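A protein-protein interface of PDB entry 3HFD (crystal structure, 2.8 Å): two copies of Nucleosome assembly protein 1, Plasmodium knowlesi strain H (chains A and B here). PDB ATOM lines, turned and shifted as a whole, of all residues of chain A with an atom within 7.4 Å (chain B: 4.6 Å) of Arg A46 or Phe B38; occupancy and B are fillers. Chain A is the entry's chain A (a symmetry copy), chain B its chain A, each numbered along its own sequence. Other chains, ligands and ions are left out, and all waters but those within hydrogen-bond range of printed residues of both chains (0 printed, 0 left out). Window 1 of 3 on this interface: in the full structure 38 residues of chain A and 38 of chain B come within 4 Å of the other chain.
Printed residues of chain B that touch a printed residue of chain A: Tyr B34, Glu B35, Lys B37, Phe B38, Glu B41 and Leu B42.
Hydrophobic or aromatic side chains of chain B within 4 Å of the printed part of chain A: Tyr B34 and Phe B38.
Hydrophobic or aromatic side chains of chain A that line the printed part of chain B: Leu A45, Tyr A49, Leu A52 and Tyr A53.
Among the printed residues, Asp or Glu carboxylates within 4 Å of a Lys or Arg side-chain nitrogen of the other chain: Lys A48 with Glu B41 (3.4 Å).
Of chain B, only Phe B38 (3.9 Å) comes within 4 Å of Arg A46.
Of the printed residues of chain B, Lys A48 touches Glu B41 (3.4 Å).
His A50 touches none of the printed residues of chain B.
Of the printed residues of chain B, Leu A52 touches Tyr B34 (3.3 Å).
Of the printed residues of chain B, Tyr A53 touches Tyr B34 and Glu B35.
Printed residues of chain A within 4 Å of Glu B35: Tyr A53 (3.6 Å).
Of chain A, only Leu A45, Arg A46 and Tyr A49 come within 4 Å of Phe B38.
Of the printed residues of chain A, Leu B42 touches Leu A45.
The nearest printed residue of chain B that does not touch Arg A46 is Leu B42 (5.7 Å).
The nearest residue of chain A that does not touch Phe B38 is Tyr A53 (4.1 Å).
The nearest printed residue of chain A that does not touch Tyr B34 is Lys A48 (7.4 Å).
The backbone carbonyl oxygen (O) of Lys B37 sits close to the side-chain hydroxyl (OH) of Tyr A49.
The backbone NH of Phe B38 lies close to the side-chain hydroxyl of Tyr A49, 3.5 Å away.
OE1 of Glu B41 is in salt-bridge range of NZ of Lys A48.
The side-chain carboxylate of Glu B41 is in hydrogen-bond range of the side-chain hydroxyl of Tyr A49, at 3.2 Å.
Among the printed residues, merely in contact across the chains: Leu A45 with Phe B38, Leu A45 with Glu B41, Leu A45 with Leu B42, Arg A46 with Phe B38, Tyr A49 with Tyr B34, Leu A52 with Tyr B34, Tyr A53 with Tyr B34 and Tyr A53 with Glu B35.
Positions printed for both chains: 38, 40, 41 and 42.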
ATOM      1  N   PHE A  38      -2.450  33.782  13.617  1.00  0.00           N
ATOM      2  CA  PHE A  38      -1.988  33.390  14.941  1.00  0.00           C
ATOM      3  C   PHE A  38      -3.040  33.705  16.005  1.00  0.00           C
ATOM      4  O   PHE A  38      -3.483  32.810  16.728  1.00  0.00           O
ATOM      5  CB  PHE A  38      -0.672  34.105  15.271  1.00  0.00           C
ATOM      6  CG  PHE A  38      -0.223  33.921  16.680  1.00  0.00           C
ATOM      7  CD1 PHE A  38       0.501  32.795  17.047  1.00  0.00           C
ATOM      8  CD2 PHE A  38      -0.532  34.868  17.650  1.00  0.00           C
ATOM      9  CE1 PHE A  38       0.919  32.611  18.362  1.00  0.00           C
ATOM     10  CE2 PHE A  38      -0.121  34.693  18.969  1.00  0.00           C
ATOM     11  CZ  PHE A  38       0.607  33.557  19.326  1.00  0.00           C
ATOM     12  N   TYR A  40      -6.092  34.107  15.718  1.00  0.00           N
ATOM     13  CA  TYR A  40      -7.217  33.196  15.533  1.00  0.00           C
ATOM     14  C   TYR A  40      -6.880  31.839  16.147  1.00  0.00           C
ATOM     15  O   TYR A  40      -7.556  31.380  17.073  1.00  0.00           O
ATOM     16  CB  TYR A  40      -7.577  33.051  14.055  1.00  0.00           C
ATOM     17  CG  TYR A  40      -8.733  32.105  13.806  1.00  0.00           C
ATOM     18  CD1 TYR A  40     -10.018  32.415  14.240  1.00  0.00           C
ATOM     19  CD2 TYR A  40      -8.539  30.903  13.134  1.00  0.00           C
ATOM     20  CE1 TYR A  40     -11.076  31.554  14.015  1.00  0.00           C
ATOM     21  CE2 TYR A  40      -9.592  30.038  12.899  1.00  0.00           C
ATOM     22  CZ  TYR A  40     -10.856  30.365  13.346  1.00  0.00           C
ATOM     23  OH  TYR A  40     -11.899  29.497  13.113  1.00  0.00           O
ATOM     24  N   GLU A  41      -5.810  31.226  15.652  1.00  0.00           N
ATOM     25  CA  GLU A  41      -5.372  29.919  16.137  1.00  0.00           C
ATOM     26  C   GLU A  41      -5.206  29.874  17.665  1.00  0.00           C
ATOM     27  O   GLU A  41      -5.614  28.910  18.294  1.00  0.00           O
ATOM     28  CB  GLU A  41      -4.080  29.478  15.416  1.00  0.00           C
ATOM     29  CG  GLU A  41      -4.313  29.153  13.927  1.00  0.00           C
ATOM     30  CD  GLU A  41      -3.268  28.231  13.296  1.00  0.00           C
ATOM     31  OE1 GLU A  41      -3.582  27.618  12.250  1.00  0.00           O
ATOM     32  OE2 GLU A  41      -2.144  28.115  13.824  1.00  0.00           O
ATOM     33  N   LEU A  42      -4.625  30.918  18.246  1.00  0.00           N
ATOM     34  CA  LEU A  42      -4.488  31.048  19.709  1.00  0.00           C
ATOM     35  C   LEU A  42      -5.836  31.054  20.404  1.00  0.00           C
ATOM     36  O   LEU A  42      -5.994  30.494  21.479  1.00  0.00           O
ATOM     37  CB  LEU A  42      -3.742  32.343  20.055  1.00  0.00           C
ATOM     38  CG  LEU A  42      -3.817  32.939  21.463  1.00  0.00           C
ATOM     39  CD1 LEU A  42      -3.143  32.048  22.485  1.00  0.00           C
ATOM     40  CD2 LEU A  42      -3.166  34.298  21.455  1.00  0.00           C
ATOM     41  N   PHE A  43      -6.808  31.696  19.775  1.00  0.00           N
ATOM     42  CA  PHE A  43      -8.142  31.823  20.345  1.00  0.00           C
ATOM     43  C   PHE A  43      -8.938  30.522  20.221  1.00  0.00           C
ATOM     44  O   PHE A  43      -9.706  30.191  21.120  1.00  0.00           O
ATOM     45  CB  PHE A  43      -8.867  33.025  19.727  1.00  0.00           C
ATOM     46  CG  PHE A  43      -8.408  34.374  20.281  1.00  0.00           C
ATOM     47  CD1 PHE A  43      -7.051  34.627  20.564  1.00  0.00           C
ATOM     48  CD2 PHE A  43      -9.334  35.393  20.513  1.00  0.00           C
ATOM     49  CE1 PHE A  43      -6.627  35.869  21.059  1.00  0.00           C
ATOM     50  CE2 PHE A  43      -8.921  36.647  21.019  1.00  0.00           C
ATOM     51  CZ  PHE A  43      -7.561  36.883  21.289  1.00  0.00           C
ATOM     52  N   LEU A  44      -8.744  29.780  19.125  1.00  0.00           N
ATOM     53  CA  LEU A  44      -9.095  28.349  19.094  1.00  0.00           C
ATOM     54  C   LEU A  44      -8.539  27.641  20.334  1.00  0.00           C
ATOM     55  O   LEU A  44      -9.277  27.104  21.157  1.00  0.00           O
ATOM     56  CB  LEU A  44      -8.497  27.660  17.861  1.00  0.00           C
ATOM     57  CG  LEU A  44      -9.200  27.748  16.510  1.00  0.00           C
ATOM     58  CD1 LEU A  44      -8.265  27.276  15.379  1.00  0.00           C
ATOM     59  CD2 LEU A  44     -10.489  26.937  16.518  1.00  0.00           C
ATOM     60  N   LEU A  45      -7.219  27.669  20.459  1.00  0.00           N
ATOM     61  CA  LEU A  45      -6.502  26.871  21.447  1.00  0.00           C
ATOM     62  C   LEU A  45      -6.951  27.128  22.880  1.00  0.00           C
ATOM     63  O   LEU A  45      -7.075  26.182  23.651  1.00  0.00           O
ATOM     64  CB  LEU A  45      -4.994  27.118  21.335  1.00  0.00           C
ATOM     65  CG  LEU A  45      -4.085  26.166  22.100  1.00  0.00           C
ATOM     66  CD1 LEU A  45      -4.595  24.751  22.010  1.00  0.00           C
ATOM     67  CD2 LEU A  45      -2.659  26.255  21.572  1.00  0.00           C
ATOM     68  N   ARG A  46      -7.180  28.394  23.233  1.00  0.00           N
ATOM     69  CA  ARG A  46      -7.672  28.744  24.572  1.00  0.00           C
ATOM     70  C   ARG A  46      -9.065  28.158  24.831  1.00  0.00           C
ATOM     71  O   ARG A  46      -9.313  27.579  25.891  1.00  0.00           O
ATOM     72  CB  ARG A  46      -7.726  30.258  24.773  1.00  0.00           C
ATOM     73  CG  ARG A  46      -6.373  30.951  24.914  1.00  0.00           C
ATOM     74  CD  ARG A  46      -6.534  32.269  25.690  1.00  0.00           C
ATOM     75  NE  ARG A  46      -5.518  33.279  25.387  1.00  0.00           N
ATOM     76  CZ  ARG A  46      -4.258  33.254  25.823  1.00  0.00           C
ATOM     77  NH1 ARG A  46      -3.804  32.256  26.584  1.00  0.00           N
ATOM     78  NH2 ARG A  46      -3.433  34.236  25.479  1.00  0.00           N
ATOM     79  N   GLN A  47      -9.972  28.315  23.871  1.00  0.00           N
ATOM     80  CA  GLN A  47     -11.312  27.759  24.005  1.00  0.00           C
ATOM     81  C   GLN A  47     -11.247  26.251  24.106  1.00  0.00           C
ATOM     82  O   GLN A  47     -11.738  25.671  25.069  1.00  0.00           O
ATOM     83  CB  GLN A  47     -12.215  28.177  22.827  1.00  0.00           C
ATOM     84  CG  GLN A  47     -12.612  29.669  22.836  1.00  0.00           C
ATOM     85  CD  GLN A  47     -12.801  30.227  24.249  1.00  0.00           C
ATOM     86  OE1 GLN A  47     -11.940  30.948  24.761  1.00  0.00           O
ATOM     87  NE2 GLN A  47     -13.911  29.854  24.897  1.00  0.00           N
ATOM     88  N   LYS A  48     -10.616  25.619  23.123  1.00  0.00           N
ATOM     89  CA  LYS A  48     -10.504  24.157  23.096  1.00  0.00           C
ATOM     90  C   LYS A  48     -10.299  23.598  24.502  1.00  0.00           C
ATOM     91  O   LYS A  48     -10.918  22.601  24.862  1.00  0.00           O
ATOM     92  CB  LYS A  48      -9.346  23.707  22.185  1.00  0.00           C
ATOM     93  CG  LYS A  48      -9.266  22.195  21.932  1.00  0.00           C
ATOM     94  CD  LYS A  48      -7.922  21.807  21.331  1.00  0.00           C
ATOM     95  CE  LYS A  48      -7.764  20.294  21.176  1.00  0.00           C
ATOM     96  NZ  LYS A  48      -6.456  19.930  20.560  1.00  0.00           N
ATOM     97  N   TYR A  49      -9.441  24.265  25.278  1.00  0.00           N
ATOM     98  CA  TYR A  49      -9.075  23.834  26.630  1.00  0.00           C
ATOM     99  C   TYR A  49      -9.972  24.388  27.748  1.00  0.00           C
ATOM    100  O   TYR A  49     -10.223  23.679  28.718  1.00  0.00           O
ATOM    101  CB  TYR A  49      -7.604  24.150  26.908  1.00  0.00           C
ATOM    102  CG  TYR A  49      -6.643  23.212  26.192  1.00  0.00           C
ATOM    103  CD1 TYR A  49      -5.950  22.225  26.888  1.00  0.00           C
ATOM    104  CD2 TYR A  49      -6.426  23.312  24.817  1.00  0.00           C
ATOM    105  CE1 TYR A  49      -5.060  21.366  26.235  1.00  0.00           C
ATOM    106  CE2 TYR A  49      -5.535  22.452  24.156  1.00  0.00           C
ATOM    107  CZ  TYR A  49      -4.857  21.481  24.872  1.00  0.00           C
ATOM    108  OH  TYR A  49      -3.986  20.631  24.223  1.00  0.00           O
ATOM    109  N   HIS A  50     -10.461  25.624  27.635  1.00  0.00           N
ATOM    110  CA  HIS A  50     -11.512  26.102  28.555  1.00  0.00           C
ATOM    111  C   HIS A  50     -12.573  25.005  28.673  1.00  0.00           C
ATOM    112  O   HIS A  50     -12.948  24.625  29.773  1.00  0.00           O
ATOM    113  CB  HIS A  50     -12.112  27.426  28.063  1.00  0.00           C
ATOM    114  CG  HIS A  50     -13.422  27.803  28.704  1.00  0.00           C
ATOM    115  ND1 HIS A  50     -13.516  28.713  29.739  1.00  0.00           N
ATOM    116  CD2 HIS A  50     -14.698  27.436  28.419  1.00  0.00           C
ATOM    117  CE1 HIS A  50     -14.785  28.866  30.085  1.00  0.00           C
ATOM    118  NE2 HIS A  50     -15.524  28.108  29.294  1.00  0.00           N
ATOM    119  N   ASP A  51     -13.013  24.481  27.530  1.00  0.00           N
ATOM    120  CA  ASP A  51     -13.941  23.348  27.479  1.00  0.00           C
ATOM    121  C   ASP A  51     -13.395  22.106  28.151  1.00  0.00           C
ATOM    122  O   ASP A  51     -14.101  21.458  28.909  1.00  0.00           O
ATOM    123  CB  ASP A  51     -14.257  22.966  26.036  1.00  0.00           C
ATOM    124  CG  ASP A  51     -15.254  23.889  25.386  1.00  0.00           C
ATOM    125  OD1 ASP A  51     -15.543  24.990  25.927  1.00  0.00           O
ATOM    126  OD2 ASP A  51     -15.753  23.496  24.310  1.00  0.00           O
ATOM    127  N   LEU A  52     -12.153  21.749  27.840  1.00  0.00           N
ATOM    128  CA  LEU A  52     -11.550  20.551  28.417  1.00  0.00           C
ATOM    129  C   LEU A  52     -11.603  20.608  29.937  1.00  0.00           C
ATOM    130  O   LEU A  52     -11.802  19.578  30.581  1.00  0.00           O
ATOM    131  CB  LEU A  52     -10.095  20.349  27.959  1.00  0.00           C
ATOM    132  CG  LEU A  52      -9.773  19.990  26.501  1.00  0.00           C
ATOM    133  CD1 LEU A  52      -8.314  19.593  26.359  1.00  0.00           C
ATOM    134  CD2 LEU A  52     -10.652  18.889  25.978  1.00  0.00           C
ATOM    135  N   TYR A  53     -11.444  21.807  30.498  1.00  0.00           N
ATOM    136  CA  TYR A  53     -11.368  21.982  31.952  1.00  0.00           C
ATOM    137  C   TYR A  53     -12.721  21.836  32.608  1.00  0.00           C
ATOM    138  O   TYR A  53     -12.872  21.050  33.520  1.00  0.00           O
ATOM    139  CB  TYR A  53     -10.774  23.348  32.319  1.00  0.00           C
ATOM    140  CG  TYR A  53      -9.363  23.597  31.811  1.00  0.00           C
ATOM    141  CD1 TYR A  53      -8.417  22.570  31.744  1.00  0.00           C
ATOM    142  CD2 TYR A  53      -8.969  24.866  31.424  1.00  0.00           C
ATOM    143  CE1 TYR A  53      -7.133  22.806  31.292  1.00  0.00           C
ATOM    144  CE2 TYR A  53      -7.691  25.111  30.964  1.00  0.00           C
ATOM    145  CZ  TYR A  53      -6.770  24.080  30.904  1.00  0.00           C
ATOM    146  OH  TYR A  53      -5.486  24.335  30.446  1.00  0.00           O
ATOM    147  N   TYR A 113     -16.877  32.974  30.068  1.00  0.00           N
ATOM    148  CA  TYR A 113     -16.801  34.056  29.080  1.00  0.00           C
ATOM    149  C   TYR A 113     -18.232  34.507  28.792  1.00  0.00           C
ATOM    150  O   TYR A 113     -19.175  33.765  29.083  1.00  0.00           O
ATOM    151  CB  TYR A 113     -16.150  33.562  27.791  1.00  0.00           C
ATOM    152  CG  TYR A 113     -14.694  33.126  27.918  1.00  0.00           C
ATOM    153  CD1 TYR A 113     -13.737  33.954  28.516  1.00  0.00           C
ATOM    154  CD2 TYR A 113     -14.264  31.896  27.404  1.00  0.00           C
ATOM    155  CE1 TYR A 113     -12.389  33.561  28.617  1.00  0.00           C
ATOM    156  CE2 TYR A 113     -12.920  31.492  27.497  1.00  0.00           C
ATOM    157  CZ  TYR A 113     -11.984  32.329  28.101  1.00  0.00           C
ATOM    158  OH  TYR A 113     -10.656  31.927  28.187  1.00  0.00           O
ATOM    159  N   TYR B  34      -3.907  18.439  31.172  1.00  0.00           N
ATOM    160  CA  TYR B  34      -4.454  19.332  30.153  1.00  0.00           C
ATOM    161  C   TYR B  34      -3.705  20.664  30.102  1.00  0.00           C
ATOM    162  O   TYR B  34      -3.492  21.205  29.029  1.00  0.00           O
ATOM    163  CB  TYR B  34      -5.962  19.546  30.345  1.00  0.00           C
ATOM    164  CG  TYR B  34      -6.767  18.351  29.907  1.00  0.00           C
ATOM    165  CD1 TYR B  34      -6.652  17.864  28.608  1.00  0.00           C
ATOM    166  CD2 TYR B  34      -7.624  17.693  30.783  1.00  0.00           C
ATOM    167  CE1 TYR B  34      -7.369  16.750  28.183  1.00  0.00           C
ATOM    168  CE2 TYR B  34      -8.352  16.564  30.368  1.00  0.00           C
ATOM    169  CZ  TYR B  34      -8.218  16.102  29.058  1.00  0.00           C
ATOM    170  OH  TYR B  34      -8.918  15.003  28.609  1.00  0.00           O
ATOM    171  N   GLU B  35      -3.277  21.170  31.249  1.00  0.00           N
ATOM    172  CA  GLU B  35      -2.525  22.413  31.267  1.00  0.00           C
ATOM    173  C   GLU B  35      -1.257  22.219  30.451  1.00  0.00           C
ATOM    174  O   GLU B  35      -0.862  23.097  29.674  1.00  0.00           O
ATOM    175  CB  GLU B  35      -2.185  22.842  32.692  1.00  0.00           C
ATOM    176  CG  GLU B  35      -1.624  24.236  32.783  1.00  0.00           C
ATOM    177  CD  GLU B  35      -1.465  24.722  34.215  1.00  0.00           C
ATOM    178  OE1 GLU B  35      -0.601  24.179  34.941  1.00  0.00           O
ATOM    179  OE2 GLU B  35      -2.181  25.671  34.607  1.00  0.00           O
ATOM    180  N   SER B  36      -0.628  21.061  30.612  1.00  0.00           N
ATOM    181  CA  SER B  36       0.598  20.773  29.883  1.00  0.00           C
ATOM    182  C   SER B  36       0.335  20.665  28.398  1.00  0.00           C
ATOM    183  O   SER B  36       1.097  21.193  27.595  1.00  0.00           O
ATOM    184  CB  SER B  36       1.270  19.495  30.391  1.00  0.00           C
ATOM    185  OG  SER B  36       2.256  19.828  31.357  1.00  0.00           O
ATOM    186  N   LYS B  37      -0.746  19.987  28.032  1.00  0.00           N
ATOM    187  CA  LYS B  37      -1.072  19.804  26.616  1.00  0.00           C
ATOM    188  C   LYS B  37      -1.235  21.158  25.931  1.00  0.00           C
ATOM    189  O   LYS B  37      -0.733  21.369  24.828  1.00  0.00           O
ATOM    190  CB  LYS B  37      -2.333  18.952  26.451  1.00  0.00           C
ATOM    191  CG  LYS B  37      -2.165  17.506  26.909  1.00  0.00           C
ATOM    192  CD  LYS B  37      -3.476  16.738  26.779  1.00  0.00           C
ATOM    193  CE  LYS B  37      -3.345  15.296  27.254  1.00  0.00           C
ATOM    194  NZ  LYS B  37      -3.350  15.213  28.738  1.00  0.00           N
ATOM    195  N   PHE B  38      -1.925  22.066  26.618  1.00  0.00           N
ATOM    196  CA  PHE B  38      -2.114  23.437  26.164  1.00  0.00           C
ATOM    197  C   PHE B  38      -0.772  24.157  26.022  1.00  0.00           C
ATOM    198  O   PHE B  38      -0.441  24.650  24.941  1.00  0.00           O
ATOM    199  CB  PHE B  38      -3.017  24.194  27.145  1.00  0.00           C
ATOM    200  CG  PHE B  38      -3.109  25.657  26.874  1.00  0.00           C
ATOM    201  CD1 PHE B  38      -4.012  26.144  25.938  1.00  0.00           C
ATOM    202  CD2 PHE B  38      -2.285  26.554  27.544  1.00  0.00           C
ATOM    203  CE1 PHE B  38      -4.100  27.508  25.673  1.00  0.00           C
ATOM    204  CE2 PHE B  38      -2.363  27.920  27.285  1.00  0.00           C
ATOM    205  CZ  PHE B  38      -3.275  28.398  26.343  1.00  0.00           C
ATOM    206  N   GLU B  39      -0.003  24.222  27.108  1.00  0.00           N
ATOM    207  CA  GLU B  39       1.320  24.853  27.052  1.00  0.00           C
ATOM    208  C   GLU B  39       2.143  24.303  25.887  1.00  0.00           C
ATOM    209  O   GLU B  39       2.838  25.057  25.215  1.00  0.00           O
ATOM    210  CB  GLU B  39       2.099  24.671  28.357  1.00  0.00           C
ATOM    211  CG  GLU B  39       1.965  25.819  29.349  1.00  0.00           C
ATOM    212  CD  GLU B  39       2.860  25.645  30.597  1.00  0.00           C
ATOM    213  OE1 GLU B  39       2.372  25.918  31.727  1.00  0.00           O
ATOM    214  OE2 GLU B  39       4.046  25.234  30.453  1.00  0.00           O
ATOM    215  N   TYR B  40       2.069  22.999  25.636  1.00  0.00           N
ATOM    216  CA  TYR B  40       2.778  22.423  24.497  1.00  0.00           C
ATOM    217  C   TYR B  40       2.226  23.014  23.202  1.00  0.00           C
ATOM    218  O   TYR B  40       2.955  23.661  22.443  1.00  0.00           O
ATOM    219  CB  TYR B  40       2.671  20.899  24.491  1.00  0.00           C
ATOM    220  CG  TYR B  40       3.381  20.251  23.321  1.00  0.00           C
ATOM    221  CD1 TYR B  40       4.767  20.301  23.207  1.00  0.00           C
ATOM    222  CD2 TYR B  40       2.665  19.586  22.331  1.00  0.00           C
ATOM    223  CE1 TYR B  40       5.419  19.711  22.141  1.00  0.00           C
ATOM    224  CE2 TYR B  40       3.310  18.988  21.264  1.00  0.00           C
ATOM    225  CZ  TYR B  40       4.684  19.058  21.170  1.00  0.00           C
ATOM    226  OH  TYR B  40       5.318  18.463  20.102  1.00  0.00           O
ATOM    227  N   GLU B  41       0.931  22.821  22.979  1.00  0.00           N
ATOM    228  CA  GLU B  41       0.268  23.323  21.778  1.00  0.00           C
ATOM    229  C   GLU B  41       0.509  24.823  21.545  1.00  0.00           C
ATOM    230  O   GLU B  41       0.762  25.233  20.423  1.00  0.00           O
ATOM    231  CB  GLU B  41      -1.240  22.992  21.813  1.00  0.00           C
ATOM    232  CG  GLU B  41      -1.520  21.483  21.669  1.00  0.00           C
ATOM    233  CD  GLU B  41      -2.921  21.131  21.166  1.00  0.00           C
ATOM    234  OE1 GLU B  41      -3.095  19.998  20.659  1.00  0.00           O
ATOM    235  OE2 GLU B  41      -3.845  21.961  21.274  1.00  0.00           O
ATOM    236  N   LEU B  42       0.443  25.622  22.604  1.00  0.00           N
ATOM    237  CA  LEU B  42       0.746  27.064  22.541  1.00  0.00           C
ATOM    238  C   LEU B  42       2.168  27.323  22.081  1.00  0.00           C
ATOM    239  O   LEU B  42       2.431  28.261  21.341  1.00  0.00           O
ATOM    240  CB  LEU B  42       0.542  27.707  23.919  1.00  0.00           C
ATOM    241  CG  LEU B  42       1.163  29.066  24.250  1.00  0.00           C
ATOM    242  CD1 LEU B  42       0.551  30.179  23.425  1.00  0.00           C
ATOM    243  CD2 LEU B  42       0.971  29.347  25.718  1.00  0.00           C
